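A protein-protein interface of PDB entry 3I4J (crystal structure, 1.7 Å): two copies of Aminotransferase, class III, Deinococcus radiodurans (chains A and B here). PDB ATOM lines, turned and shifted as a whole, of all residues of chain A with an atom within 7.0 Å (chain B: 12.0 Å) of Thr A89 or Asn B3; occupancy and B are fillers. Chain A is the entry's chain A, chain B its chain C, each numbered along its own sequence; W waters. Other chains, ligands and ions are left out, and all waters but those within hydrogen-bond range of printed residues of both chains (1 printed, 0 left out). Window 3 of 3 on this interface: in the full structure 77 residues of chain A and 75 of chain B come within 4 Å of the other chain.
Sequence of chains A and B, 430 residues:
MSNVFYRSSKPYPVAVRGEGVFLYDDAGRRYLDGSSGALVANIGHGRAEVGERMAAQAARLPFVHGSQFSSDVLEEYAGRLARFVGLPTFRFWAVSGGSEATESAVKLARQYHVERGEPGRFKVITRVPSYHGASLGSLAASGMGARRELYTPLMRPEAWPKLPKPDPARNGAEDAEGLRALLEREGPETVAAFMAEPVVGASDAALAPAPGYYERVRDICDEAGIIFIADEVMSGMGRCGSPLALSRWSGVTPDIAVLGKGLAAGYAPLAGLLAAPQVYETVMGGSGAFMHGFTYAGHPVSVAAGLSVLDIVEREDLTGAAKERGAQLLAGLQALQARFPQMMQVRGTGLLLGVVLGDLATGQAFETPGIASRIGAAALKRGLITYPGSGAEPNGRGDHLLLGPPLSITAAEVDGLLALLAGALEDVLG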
ATOM      1  N   LEU A  74      33.059 -10.654  17.205  1.00  0.00           N
ATOM      2  CA  LEU A  74      32.023 -11.381  16.475  1.00  0.00           C
ATOM      3  C   LEU A  74      30.754 -10.522  16.395  1.00  0.00           C
ATOM      4  O   LEU A  74      30.092 -10.487  15.356  1.00  0.00           O
ATOM      5  CB  LEU A  74      31.703 -12.718  17.152  1.00  0.00           C
ATOM      6  CG  LEU A  74      30.547 -13.524  16.541  1.00  0.00           C
ATOM      7  CD1 LEU A  74      30.852 -13.886  15.084  1.00  0.00           C
ATOM      8  CD2 LEU A  74      30.334 -14.790  17.376  1.00  0.00           C
ATOM      9  N   GLU A  75      30.422  -9.831  17.485  1.00  0.00           N
ATOM     10  CA  GLU A  75      29.242  -8.968  17.496  1.00  0.00           C
ATOM     11  C   GLU A  75      29.419  -7.885  16.424  1.00  0.00           C
ATOM     12  O   GLU A  75      28.490  -7.567  15.686  1.00  0.00           O
ATOM     13  CB  GLU A  75      29.069  -8.297  18.864  1.00  0.00           C
ATOM     14  CG  GLU A  75      28.792  -9.240  20.036  1.00  0.00           C
ATOM     15  CD  GLU A  75      27.419  -9.880  19.983  1.00  0.00           C
ATOM     16  OE1 GLU A  75      26.486  -9.257  19.423  1.00  0.00           O
ATOM     17  OE2 GLU A  75      27.266 -11.000  20.521  1.00  0.00           O
ATOM     18  N   GLU A  76      30.623  -7.326  16.348  1.00  0.00           N
ATOM     19  CA  GLU A  76      30.924  -6.278  15.370  1.00  0.00           C
ATOM     20  C   GLU A  76      30.843  -6.833  13.947  1.00  0.00           C
ATOM     21  O   GLU A  76      30.133  -6.294  13.090  1.00  0.00           O
ATOM     22  CB  GLU A  76      32.324  -5.704  15.626  1.00  0.00           C
ATOM     23  CG  GLU A  76      32.779  -4.661  14.599  1.00  0.00           C
ATOM     24  CD  GLU A  76      34.130  -4.035  14.934  1.00  0.00           C
ATOM     25  OE1 GLU A  76      34.804  -4.513  15.871  1.00  0.00           O
ATOM     26  OE2 GLU A  76      34.522  -3.064  14.252  1.00  0.00           O
ATOM     27  N   TYR A  77      31.569  -7.918  13.703  1.00  0.00           N
ATOM     28  CA  TYR A  77      31.597  -8.541  12.386  1.00  0.00           C
ATOM     29  C   TYR A  77      30.218  -8.978  11.893  1.00  0.00           C
ATOM     30  O   TYR A  77      29.874  -8.761  10.737  1.00  0.00           O
ATOM     31  CB  TYR A  77      32.540  -9.748  12.397  1.00  0.00           C
ATOM     32  CG  TYR A  77      32.666 -10.433  11.056  1.00  0.00           C
ATOM     33  CD1 TYR A  77      33.126  -9.734   9.936  1.00  0.00           C
ATOM     34  CD2 TYR A  77      32.340 -11.780  10.905  1.00  0.00           C
ATOM     35  CE1 TYR A  77      33.261 -10.355   8.700  1.00  0.00           C
ATOM     36  CE2 TYR A  77      32.471 -12.415   9.668  1.00  0.00           C
ATOM     37  CZ  TYR A  77      32.935 -11.695   8.571  1.00  0.00           C
ATOM     38  OH  TYR A  77      33.077 -12.313   7.354  1.00  0.00           O
ATOM     39  N   ALA A  78      29.428  -9.598  12.764  1.00  0.00           N
ATOM     40  CA  ALA A  78      28.101 -10.057  12.371  1.00  0.00           C
ATOM     41  C   ALA A  78      27.277  -8.928  11.759  1.00  0.00           C
ATOM     42  O   ALA A  78      26.647  -9.102  10.710  1.00  0.00           O
ATOM     43  CB  ALA A  78      27.378 -10.639  13.562  1.00  0.00           C
ATOM     44  N   GLY A  79      27.292  -7.772  12.414  1.00  0.00           N
ATOM     45  CA  GLY A  79      26.537  -6.638  11.910  1.00  0.00           C
ATOM     46  C   GLY A  79      27.105  -6.094  10.610  1.00  0.00           C
ATOM     47  O   GLY A  79      26.359  -5.817   9.678  1.00  0.00           O
ATOM     48  N   ARG A  80      28.426  -5.945  10.546  1.00  0.00           N
ATOM     49  CA  ARG A  80      29.092  -5.426   9.347  1.00  0.00           C
ATOM     50  C   ARG A  80      28.849  -6.309   8.124  1.00  0.00           C
ATOM     51  O   ARG A  80      28.564  -5.811   7.038  1.00  0.00           O
ATOM     52  CB  ARG A  80      30.601  -5.305   9.594  1.00  0.00           C
ATOM     53  CG  ARG A  80      31.023  -4.137  10.497  1.00  0.00           C
ATOM     54  CD  ARG A  80      30.969  -2.809   9.740  1.00  0.00           C
ATOM     55  NE  ARG A  80      31.738  -2.881   8.499  1.00  0.00           N
ATOM     56  CZ  ARG A  80      33.065  -2.887   8.431  1.00  0.00           C
ATOM     57  NH1 ARG A  80      33.800  -2.809   9.537  1.00  0.00           N
ATOM     58  NH2 ARG A  80      33.664  -3.002   7.252  1.00  0.00           N
ATOM     59  N   ALA A  82      26.404  -8.621   7.689  1.00  0.00           N
ATOM     60  CA  ALA A  82      24.984  -8.599   7.374  1.00  0.00           C
ATOM     61  C   ALA A  82      24.667  -7.383   6.519  1.00  0.00           C
ATOM     62  O   ALA A  82      23.976  -7.494   5.514  1.00  0.00           O
ATOM     63  CB  ALA A  82      24.168  -8.567   8.655  1.00  0.00           C
ATOM     64  N   ARG A  83      25.173  -6.225   6.926  1.00  0.00           N
ATOM     65  CA  ARG A  83      24.935  -4.998   6.171  1.00  0.00           C
ATOM     66  C   ARG A  83      25.569  -5.051   4.782  1.00  0.00           C
ATOM     67  O   ARG A  83      24.928  -4.713   3.788  1.00  0.00           O
ATOM     68  CB  ARG A  83      25.458  -3.777   6.940  1.00  0.00           C
ATOM     69  CG  ARG A  83      24.634  -3.416   8.171  1.00  0.00           C
ATOM     70  CD  ARG A  83      25.058  -2.073   8.764  1.00  0.00           C
ATOM     71  NE  ARG A  83      26.348  -2.125   9.451  1.00  0.00           N
ATOM     72  CZ  ARG A  83      26.539  -2.661  10.654  1.00  0.00           C
ATOM     73  NH1 ARG A  83      25.524  -3.201  11.322  1.00  0.00           N
ATOM     74  NH2 ARG A  83      27.748  -2.650  11.199  1.00  0.00           N
ATOM     75  N   GLY A  86      23.610  -7.067   2.142  1.00  0.00           N
ATOM     76  CA  GLY A  86      22.236  -6.686   1.876  1.00  0.00           C
ATOM     77  C   GLY A  86      21.203  -7.432   2.700  1.00  0.00           C
ATOM     78  O   GLY A  86      20.019  -7.441   2.354  1.00  0.00           O
ATOM     79  N   LEU A  87      21.645  -8.063   3.786  1.00  0.00           N
ATOM     80  CA  LEU A  87      20.754  -8.799   4.685  1.00  0.00           C
ATOM     81  C   LEU A  87      21.057  -8.262   6.083  1.00  0.00           C
ATOM     82  O   LEU A  87      21.362  -9.017   7.007  1.00  0.00           O
ATOM     83  CB  LEU A  87      21.063 -10.300   4.616  1.00  0.00           C
ATOM     84  CG  LEU A  87      21.001 -10.941   3.230  1.00  0.00           C
ATOM     85  CD1 LEU A  87      21.487 -12.399   3.326  1.00  0.00           C
ATOM     86  CD2 LEU A  87      19.573 -10.881   2.699  1.00  0.00           C
ATOM     87  N   PRO A  88      20.959  -6.933   6.258  1.00  0.00           N
ATOM     88  CA  PRO A  88      21.232  -6.237   7.516  1.00  0.00           C
ATOM     89  C   PRO A  88      20.630  -6.727   8.828  1.00  0.00           C
ATOM     90  O   PRO A  88      21.253  -6.560   9.876  1.00  0.00           O
ATOM     91  CB  PRO A  88      20.846  -4.787   7.197  1.00  0.00           C
ATOM     92  CG  PRO A  88      19.775  -4.943   6.186  1.00  0.00           C
ATOM     93  CD  PRO A  88      20.360  -6.001   5.284  1.00  0.00           C
ATOM     94  N   THR A  89      19.438  -7.312   8.793  1.00  0.00           N
ATOM     95  CA  THR A  89      18.819  -7.785  10.030  1.00  0.00           C
ATOM     96  C   THR A  89      19.026  -9.279  10.286  1.00  0.00           C
ATOM     97  O   THR A  89      18.602  -9.794  11.326  1.00  0.00           O
ATOM     98  CB  THR A  89      17.299  -7.515  10.044  1.00  0.00           C
ATOM     99  OG1 THR A  89      16.653  -8.351   9.079  1.00  0.00           O
ATOM    100  CG2 THR A  89      17.013  -6.041   9.713  1.00  0.00           C
ATOM    101  N   PHE A  90      19.675  -9.968   9.352  1.00  0.00           N
ATOM    102  CA  PHE A  90      19.901 -11.410   9.490  1.00  0.00           C
ATOM    103  C   PHE A  90      20.900 -11.783  10.581  1.00  0.00           C
ATOM    104  O   PHE A  90      21.760 -10.989  10.962  1.00  0.00           O
ATOM    105  CB  PHE A  90      20.352 -12.005   8.151  1.00  0.00           C
ATOM    106  CG  PHE A  90      19.229 -12.216   7.169  1.00  0.00           C
ATOM    107  CD1 PHE A  90      18.269 -11.228   6.958  1.00  0.00           C
ATOM    108  CD2 PHE A  90      19.146 -13.390   6.434  1.00  0.00           C
ATOM    109  CE1 PHE A  90      17.242 -11.410   6.022  1.00  0.00           C
ATOM    110  CE2 PHE A  90      18.127 -13.584   5.496  1.00  0.00           C
ATOM    111  CZ  PHE A  90      17.174 -12.592   5.290  1.00  0.00           C
ATOM    112  N   ARG A  91      20.776 -13.015  11.070  1.00  0.00           N
ATOM    113  CA  ARG A  91      21.630 -13.523  12.141  1.00  0.00           C
ATOM    114  C   ARG A  91      22.750 -14.393  11.592  1.00  0.00           C
ATOM    115  O   ARG A  91      22.501 -15.341  10.850  1.00  0.00           O
ATOM    116  CB  ARG A  91      20.783 -14.322  13.127  1.00  0.00           C
ATOM    117  CG  ARG A  91      19.759 -13.479  13.880  1.00  0.00           C
ATOM    118  CD  ARG A  91      20.361 -12.879  15.141  1.00  0.00           C
ATOM    119  NE  ARG A  91      19.389 -12.062  15.865  1.00  0.00           N
ATOM    120  CZ  ARG A  91      19.529 -11.671  17.128  1.00  0.00           C
ATOM    121  NH1 ARG A  91      20.606 -12.021  17.825  1.00  0.00           N
ATOM    122  NH2 ARG A  91      18.589 -10.926  17.696  1.00  0.00           N
ATOM    123  N   PHE A  92      23.976 -14.067  11.994  1.00  0.00           N
ATOM    124  CA  PHE A  92      25.174 -14.761  11.534  1.00  0.00           C
ATOM    125  C   PHE A  92      25.618 -15.909  12.431  1.00  0.00           C
ATOM    126  O   PHE A  92      25.866 -15.725  13.627  1.00  0.00           O
ATOM    127  CB  PHE A  92      26.319 -13.749  11.391  1.00  0.00           C
ATOM    128  CG  PHE A  92      27.602 -14.343  10.863  1.00  0.00           C
ATOM    129  CD1 PHE A  92      27.622 -15.016   9.645  1.00  0.00           C
ATOM    130  CD2 PHE A  92      28.786 -14.224  11.587  1.00  0.00           C
ATOM    131  CE1 PHE A  92      28.806 -15.568   9.150  1.00  0.00           C
ATOM    132  CE2 PHE A  92      29.982 -14.769  11.104  1.00  0.00           C
ATOM    133  CZ  PHE A  92      29.991 -15.446   9.883  1.00  0.00           C
ATOM    134  N   TRP A  93      25.721 -17.087  11.825  1.00  0.00           N
ATOM    135  CA  TRP A  93      26.155 -18.315  12.487  1.00  0.00           C
ATOM    136  C   TRP A  93      27.525 -18.646  11.896  1.00  0.00           C
ATOM    137  O   TRP A  93      27.628 -19.110  10.758  1.00  0.00           O
ATOM    138  CB  TRP A  93      25.155 -19.432  12.188  1.00  0.00           C
ATOM    139  CG  TRP A  93      25.582 -20.794  12.646  1.00  0.00           C
ATOM    140  CD1 TRP A  93      25.998 -21.829  11.860  1.00  0.00           C
ATOM    141  CD2 TRP A  93      25.607 -21.275  13.991  1.00  0.00           C
ATOM    142  NE1 TRP A  93      26.277 -22.930  12.632  1.00  0.00           N
ATOM    143  CE2 TRP A  93      26.045 -22.619  13.946  1.00  0.00           C
ATOM    144  CE3 TRP A  93      25.303 -20.703  15.233  1.00  0.00           C
ATOM    145  CZ2 TRP A  93      26.184 -23.402  15.098  1.00  0.00           C
ATOM    146  CZ3 TRP A  93      25.440 -21.480  16.381  1.00  0.00           C
ATOM    147  CH2 TRP A  93      25.876 -22.818  16.304  1.00  0.00           C
ATOM    148  N   LEU A 273      26.611 -18.786   7.977  1.00  0.00           N
ATOM    149  CA  LEU A 273      25.338 -18.560   7.317  1.00  0.00           C
ATOM    150  C   LEU A 273      24.640 -17.377   7.967  1.00  0.00           C
ATOM    151  O   LEU A 273      24.923 -17.022   9.117  1.00  0.00           O
ATOM    152  CB  LEU A 273      24.451 -19.812   7.396  1.00  0.00           C
ATOM    153  CG  LEU A 273      23.953 -20.360   8.741  1.00  0.00           C
ATOM    154  CD1 LEU A 273      22.808 -19.501   9.295  1.00  0.00           C
ATOM    155  CD2 LEU A 273      23.465 -21.794   8.516  1.00  0.00           C
ATOM    156  N   LEU A 274      23.761 -16.741   7.200  1.00  0.00           N
ATOM    157  CA  LEU A 274      22.977 -15.613   7.681  1.00  0.00           C
ATOM    158  C   LEU A 274      21.545 -16.100   7.568  1.00  0.00           C
ATOM    159  O   LEU A 274      21.116 -16.525   6.500  1.00  0.00           O
ATOM    160  CB  LEU A 274      23.204 -14.377   6.797  1.00  0.00           C
ATOM    161  CG  LEU A 274      24.481 -13.583   7.098  1.00  0.00           C
ATOM    162  CD1 LEU A 274      24.771 -12.600   5.975  1.00  0.00           C
ATOM    163  CD2 LEU A 274      24.321 -12.851   8.417  1.00  0.00           C
ATOM    164  N   ALA A 275      20.828 -16.069   8.684  1.00  0.00           N
ATOM    165  CA  ALA A 275      19.450 -16.536   8.722  1.00  0.00           C
ATOM    166  C   ALA A 275      18.479 -15.390   8.967  1.00  0.00           C
ATOM    167  O   ALA A 275      18.737 -14.504   9.781  1.00  0.00           O
ATOM    168  CB  ALA A 275      19.293 -17.577   9.814  1.00  0.00           C
ATOM    169  N   ALA A 276      17.352 -15.421   8.271  1.00  0.00           N
ATOM    170  CA  ALA A 276      16.347 -14.382   8.443  1.00  0.00           C
ATOM    171  C   ALA A 276      15.852 -14.400   9.893  1.00  0.00           C
ATOM    172  O   ALA A 276      15.764 -15.459  10.522  1.00  0.00           O
ATOM    173  CB  ALA A 276      15.186 -14.624   7.483  1.00  0.00           C
ATOM    174  N   PRO A 277      15.524 -13.223  10.443  1.00  0.00           N
ATOM    175  CA  PRO A 277      15.037 -13.115  11.820  1.00  0.00           C
ATOM    176  C   PRO A 277      13.941 -14.137  12.110  1.00  0.00           C
ATOM    177  O   PRO A 277      13.910 -14.736  13.179  1.00  0.00           O
ATOM    178  CB  PRO A 277      14.519 -11.685  11.885  1.00  0.00           C
ATOM    179  CG  PRO A 277      15.449 -10.962  10.979  1.00  0.00           C
ATOM    180  CD  PRO A 277      15.556 -11.898   9.794  1.00  0.00           C
ATOM    181  N   ASN B   3      23.468  -9.031  15.777  1.00  0.00           N
ATOM    182  CA  ASN B   3      23.282  -9.863  14.551  1.00  0.00           C
ATOM    183  C   ASN B   3      23.920 -11.241  14.711  1.00  0.00           C
ATOM    184  O   ASN B   3      24.105 -11.950  13.727  1.00  0.00           O
ATOM    185  CB  ASN B   3      23.897  -9.181  13.319  1.00  0.00           C
ATOM    186  CG  ASN B   3      23.064  -8.015  12.813  1.00  0.00           C
ATOM    187  OD1 ASN B   3      23.180  -6.892  13.303  1.00  0.00           O
ATOM    188  ND2 ASN B   3      22.208  -8.285  11.833  1.00  0.00           N
ATOM    189  N   VAL B   4      24.258 -11.616  15.941  1.00  0.00           N
ATOM    190  CA  VAL B   4      24.870 -12.923  16.177  1.00  0.00           C
ATOM    191  C   VAL B   4      23.822 -14.020  16.361  1.00  0.00           C
ATOM    192  O   VAL B   4      22.835 -13.839  17.078  1.00  0.00           O
ATOM    193  CB  VAL B   4      25.801 -12.887  17.425  1.00  0.00           C
ATOM    194  CG1 VAL B   4      26.301 -14.309  17.763  1.00  0.00           C
ATOM    195  CG2 VAL B   4      26.981 -11.966  17.160  1.00  0.00           C
ATOM    196  N   PHE B   5      24.029 -15.154  15.693  1.00  0.00           N
ATOM    197  CA  PHE B   5      23.124 -16.287  15.825  1.00  0.00           C
ATOM    198  C   PHE B   5      23.690 -17.075  17.004  1.00  0.00           C
ATOM    199  O   PHE B   5      24.632 -17.855  16.847  1.00  0.00           O
ATOM    200  CB  PHE B   5      23.146 -17.126  14.540  1.00  0.00           C
ATOM    201  CG  PHE B   5      22.029 -18.136  14.439  1.00  0.00           C
ATOM    202  CD1 PHE B   5      21.281 -18.236  13.270  1.00  0.00           C
ATOM    203  CD2 PHE B   5      21.747 -19.005  15.493  1.00  0.00           C
ATOM    204  CE1 PHE B   5      20.269 -19.186  13.144  1.00  0.00           C
ATOM    205  CE2 PHE B   5      20.738 -19.962  15.378  1.00  0.00           C
ATOM    206  CZ  PHE B   5      19.997 -20.052  14.199  1.00  0.00           C
ATOM    207  N   TYR B   6      23.145 -16.836  18.195  1.00  0.00           N
ATOM    208  CA  TYR B   6      23.619 -17.522  19.392  1.00  0.00           C
ATOM    209  C   TYR B   6      23.219 -18.998  19.374  1.00  0.00           C
ATOM    210  O   TYR B   6      22.236 -19.370  18.739  1.00  0.00           O
ATOM    211  CB  TYR B   6      23.062 -16.831  20.642  1.00  0.00           C
ATOM    212  CG  TYR B   6      23.493 -15.381  20.779  1.00  0.00           C
ATOM    213  CD1 TYR B   6      24.826 -15.047  21.013  1.00  0.00           C
ATOM    214  CD2 TYR B   6      22.563 -14.342  20.676  1.00  0.00           C
ATOM    215  CE1 TYR B   6      25.227 -13.711  21.146  1.00  0.00           C
ATOM    216  CE2 TYR B   6      22.952 -13.005  20.804  1.00  0.00           C
ATOM    217  CZ  TYR B   6      24.283 -12.697  21.040  1.00  0.00           C
ATOM    218  OH  TYR B   6      24.667 -11.383  21.190  1.00  0.00           O
ATOM    219  N   ARG B   7      23.990 -19.831  20.070  1.00  0.00           N
ATOM    220  CA  ARG B   7      23.719 -21.268  20.125  1.00  0.00           C
ATOM    221  C   ARG B   7      22.416 -21.621  20.846  1.00  0.00           C
ATOM    222  O   ARG B   7      21.868 -22.708  20.652  1.00  0.00           O
ATOM    223  CB  ARG B   7      24.878 -22.004  20.797  1.00  0.00           C
ATOM    224  CG  ARG B   7      26.171 -22.028  19.993  1.00  0.00           C
ATOM    225  CD  ARG B   7      27.246 -22.766  20.759  1.00  0.00           C
ATOM    226  NE  ARG B   7      28.530 -22.810  20.061  1.00  0.00           N
ATOM    227  CZ  ARG B   7      28.975 -23.849  19.360  1.00  0.00           C
ATOM    228  NH1 ARG B   7      28.242 -24.950  19.247  1.00  0.00           N
ATOM    229  NH2 ARG B   7      30.170 -23.794  18.788  1.00  0.00           N
ATOM    230  N   SER B   8      21.928 -20.711  21.684  1.00  0.00           N
ATOM    231  CA  SER B   8      20.685 -20.947  22.414  1.00  0.00           C
ATOM    232  C   SER B   8      20.091 -19.636  22.913  1.00  0.00           C
ATOM    233  O   SER B   8      20.678 -18.571  22.724  1.00  0.00           O
ATOM    234  CB  SER B   8      20.926 -21.882  23.598  1.00  0.00           C
ATOM    235  OG  SER B   8      21.565 -21.201  24.660  1.00  0.00           O
ATOM    236  N   TYR B  12      24.373 -14.869  26.641  1.00  0.00           N
ATOM    237  CA  TYR B  12      25.784 -15.136  26.389  1.00  0.00           C
ATOM    238  C   TYR B  12      26.626 -13.907  26.699  1.00  0.00           C
ATOM    239  O   TYR B  12      26.479 -12.868  26.059  1.00  0.00           O
ATOM    240  CB  TYR B  12      25.989 -15.546  24.928  1.00  0.00           C
ATOM    241  CG  TYR B  12      25.523 -16.951  24.636  1.00  0.00           C
ATOM    242  CD1 TYR B  12      26.336 -18.048  24.921  1.00  0.00           C
ATOM    243  CD2 TYR B  12      24.245 -17.189  24.143  1.00  0.00           C
ATOM    244  CE1 TYR B  12      25.881 -19.354  24.731  1.00  0.00           C
ATOM    245  CE2 TYR B  12      23.779 -18.483  23.952  1.00  0.00           C
ATOM    246  CZ  TYR B  12      24.599 -19.562  24.252  1.00  0.00           C
ATOM    247  OH  TYR B  12      24.115 -20.840  24.104  1.00  0.00           O
ATOM    248  N   VAL B  14      29.572 -11.283  26.632  1.00  0.00           N
ATOM    249  CA  VAL B  14      30.433 -10.904  25.517  1.00  0.00           C
ATOM    250  C   VAL B  14      31.874 -10.733  25.979  1.00  0.00           C
ATOM    251  O   VAL B  14      32.199  -9.790  26.705  1.00  0.00           O
ATOM    252  CB  VAL B  14      29.956  -9.590  24.864  1.00  0.00           C
ATOM    253  CG1 VAL B  14      30.882  -9.210  23.710  1.00  0.00           C
ATOM    254  CG2 VAL B  14      28.527  -9.753  24.363  1.00  0.00           C
HETATM  255  O   HOH W   1      25.973  -8.198  16.673  1.00  0.00           O
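No position is printed for both chains.
Hydrophobic or aromatic side chains of chain A that line the printed part of chain B: Leu A74, Ala A78, Ala A82, Phe A92, Trp A93 and Ala A275.
Along chain A the printed residues that touch a printed residue of chain B span positions 74 to 275.
Among the printed residues, 20 pairs touch across the chains.
Among the printed residues, no Asp or Glu carboxylate lies within 4 Å of a Lys or Arg side-chain nitrogen of the other chain.
Water W1 bridges O of Glu A75 and N of Asn B3.
Of chain B, only Asn B3 (3.6 Å) comes within 4 Å of Gly A79.
No residue of chain B comes within 4 Å of Arg A83.
No residue of chain B comes within 4 Å of Gly A86.
Leu A87 touches none of the printed residues of chain B.
Thr A89 touches just one residue of chain B: Asn B3.
Arg A91 touches just these residues of chain B: Asn B3, Val B4, Phe B5 and Tyr B6.
Of the printed residues of chain B, Ala A275 touches Phe B5.
No residue of chain B comes within 4 Å of Ala A276.
No residue of chain B comes within 4 Å of Pro A277.
Asn B3 touches just these residues of chain A: Ala A78, Gly A79, Ala A82, Pro A88, Thr A89, Phe A90, Arg A91 and Phe A92.
Printed residues of chain A within 4 Å of Val B4: Leu A74 (3.9 Å), Glu A75 (3.5 Å), Ala A78 (3.9 Å), Arg A91 (3.0 Å) and Phe A92 (3.8 Å).
Of the printed residues of chain A, Phe B5 touches Arg A91 (3.9 Å), Phe A92 (2.8 Å), Trp A93 (3.3 Å) and Ala A275 (3.8 Å).
Of the printed residues of chain A, Arg B7 touches Trp A93 (3.7 Å).
The nearest residue of chain B that does not touch Thr A89 is Val B4 (7.5 Å).
The nearest printed residue of chain B that does not touch Ala A275 is Asn B3 (7.1 Å).
Val B4 touches Leu A74.
CB of Ala A78 touches O of Asn B3 (3.5 Å).
Ala A78 touches Val B4.
Gly A79 touches Asn B3.
Ala A82 touches Asn B3.
Asn B3 touches Thr A89.
CB of Arg A91 touches CB of Phe B5 (3.9 Å).
Tyr B6 touches Arg A91 (CE2 to NH1, 3.9 Å).
Phe B5 touches Trp A93 (O to CE3, 3.3 Å).
CZ3 of Trp A93 touches CG of Arg B7, 3.7 Å away.
The side-chain carboxylate (OE2) of Glu A75 sits at hydrogen-bond distance from the side-chain hydroxyl (OH) of Tyr B6.
The side-chain amide nitrogen (ND2) of Asn B3 lies within hydrogen-bond range of the backbone carbonyl oxygen (O) of Pro A88, at 2.8 Å.
The backbone carbonyl oxygen of Phe A90 is in hydrogen-bond range of the side-chain amide nitrogen of Asn B3 (2.9 Å).
The guanidinium group of Arg A91 sits at hydrogen-bond distance from the backbone carbonyl oxygen of Val B4, at 3.0 Å.
The backbone NH (N) of Phe A92 sits at hydrogen-bond distance from the backbone carbonyl oxygen (O) of Asn B3 (2.7 Å).
The backbone carbonyl oxygen (O) of Phe A92 is in hydrogen-bond range of the backbone NH (N) of Phe B5 (2.8 Å).
The guanidinium group (NH1) of Arg A83 is in hydrogen-bond range of the backbone carbonyl oxygen (O) of Gly A79.
O of Ala A82 lies within hydrogen-bond range of N of Leu A87 (3.0 Å).
O of Arg A91 sits at hydrogen-bond distance from N of Ala A275, at 2.8 Å.
O of Leu A273 lies within hydrogen-bond range of N of Trp A93 (2.8 Å).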
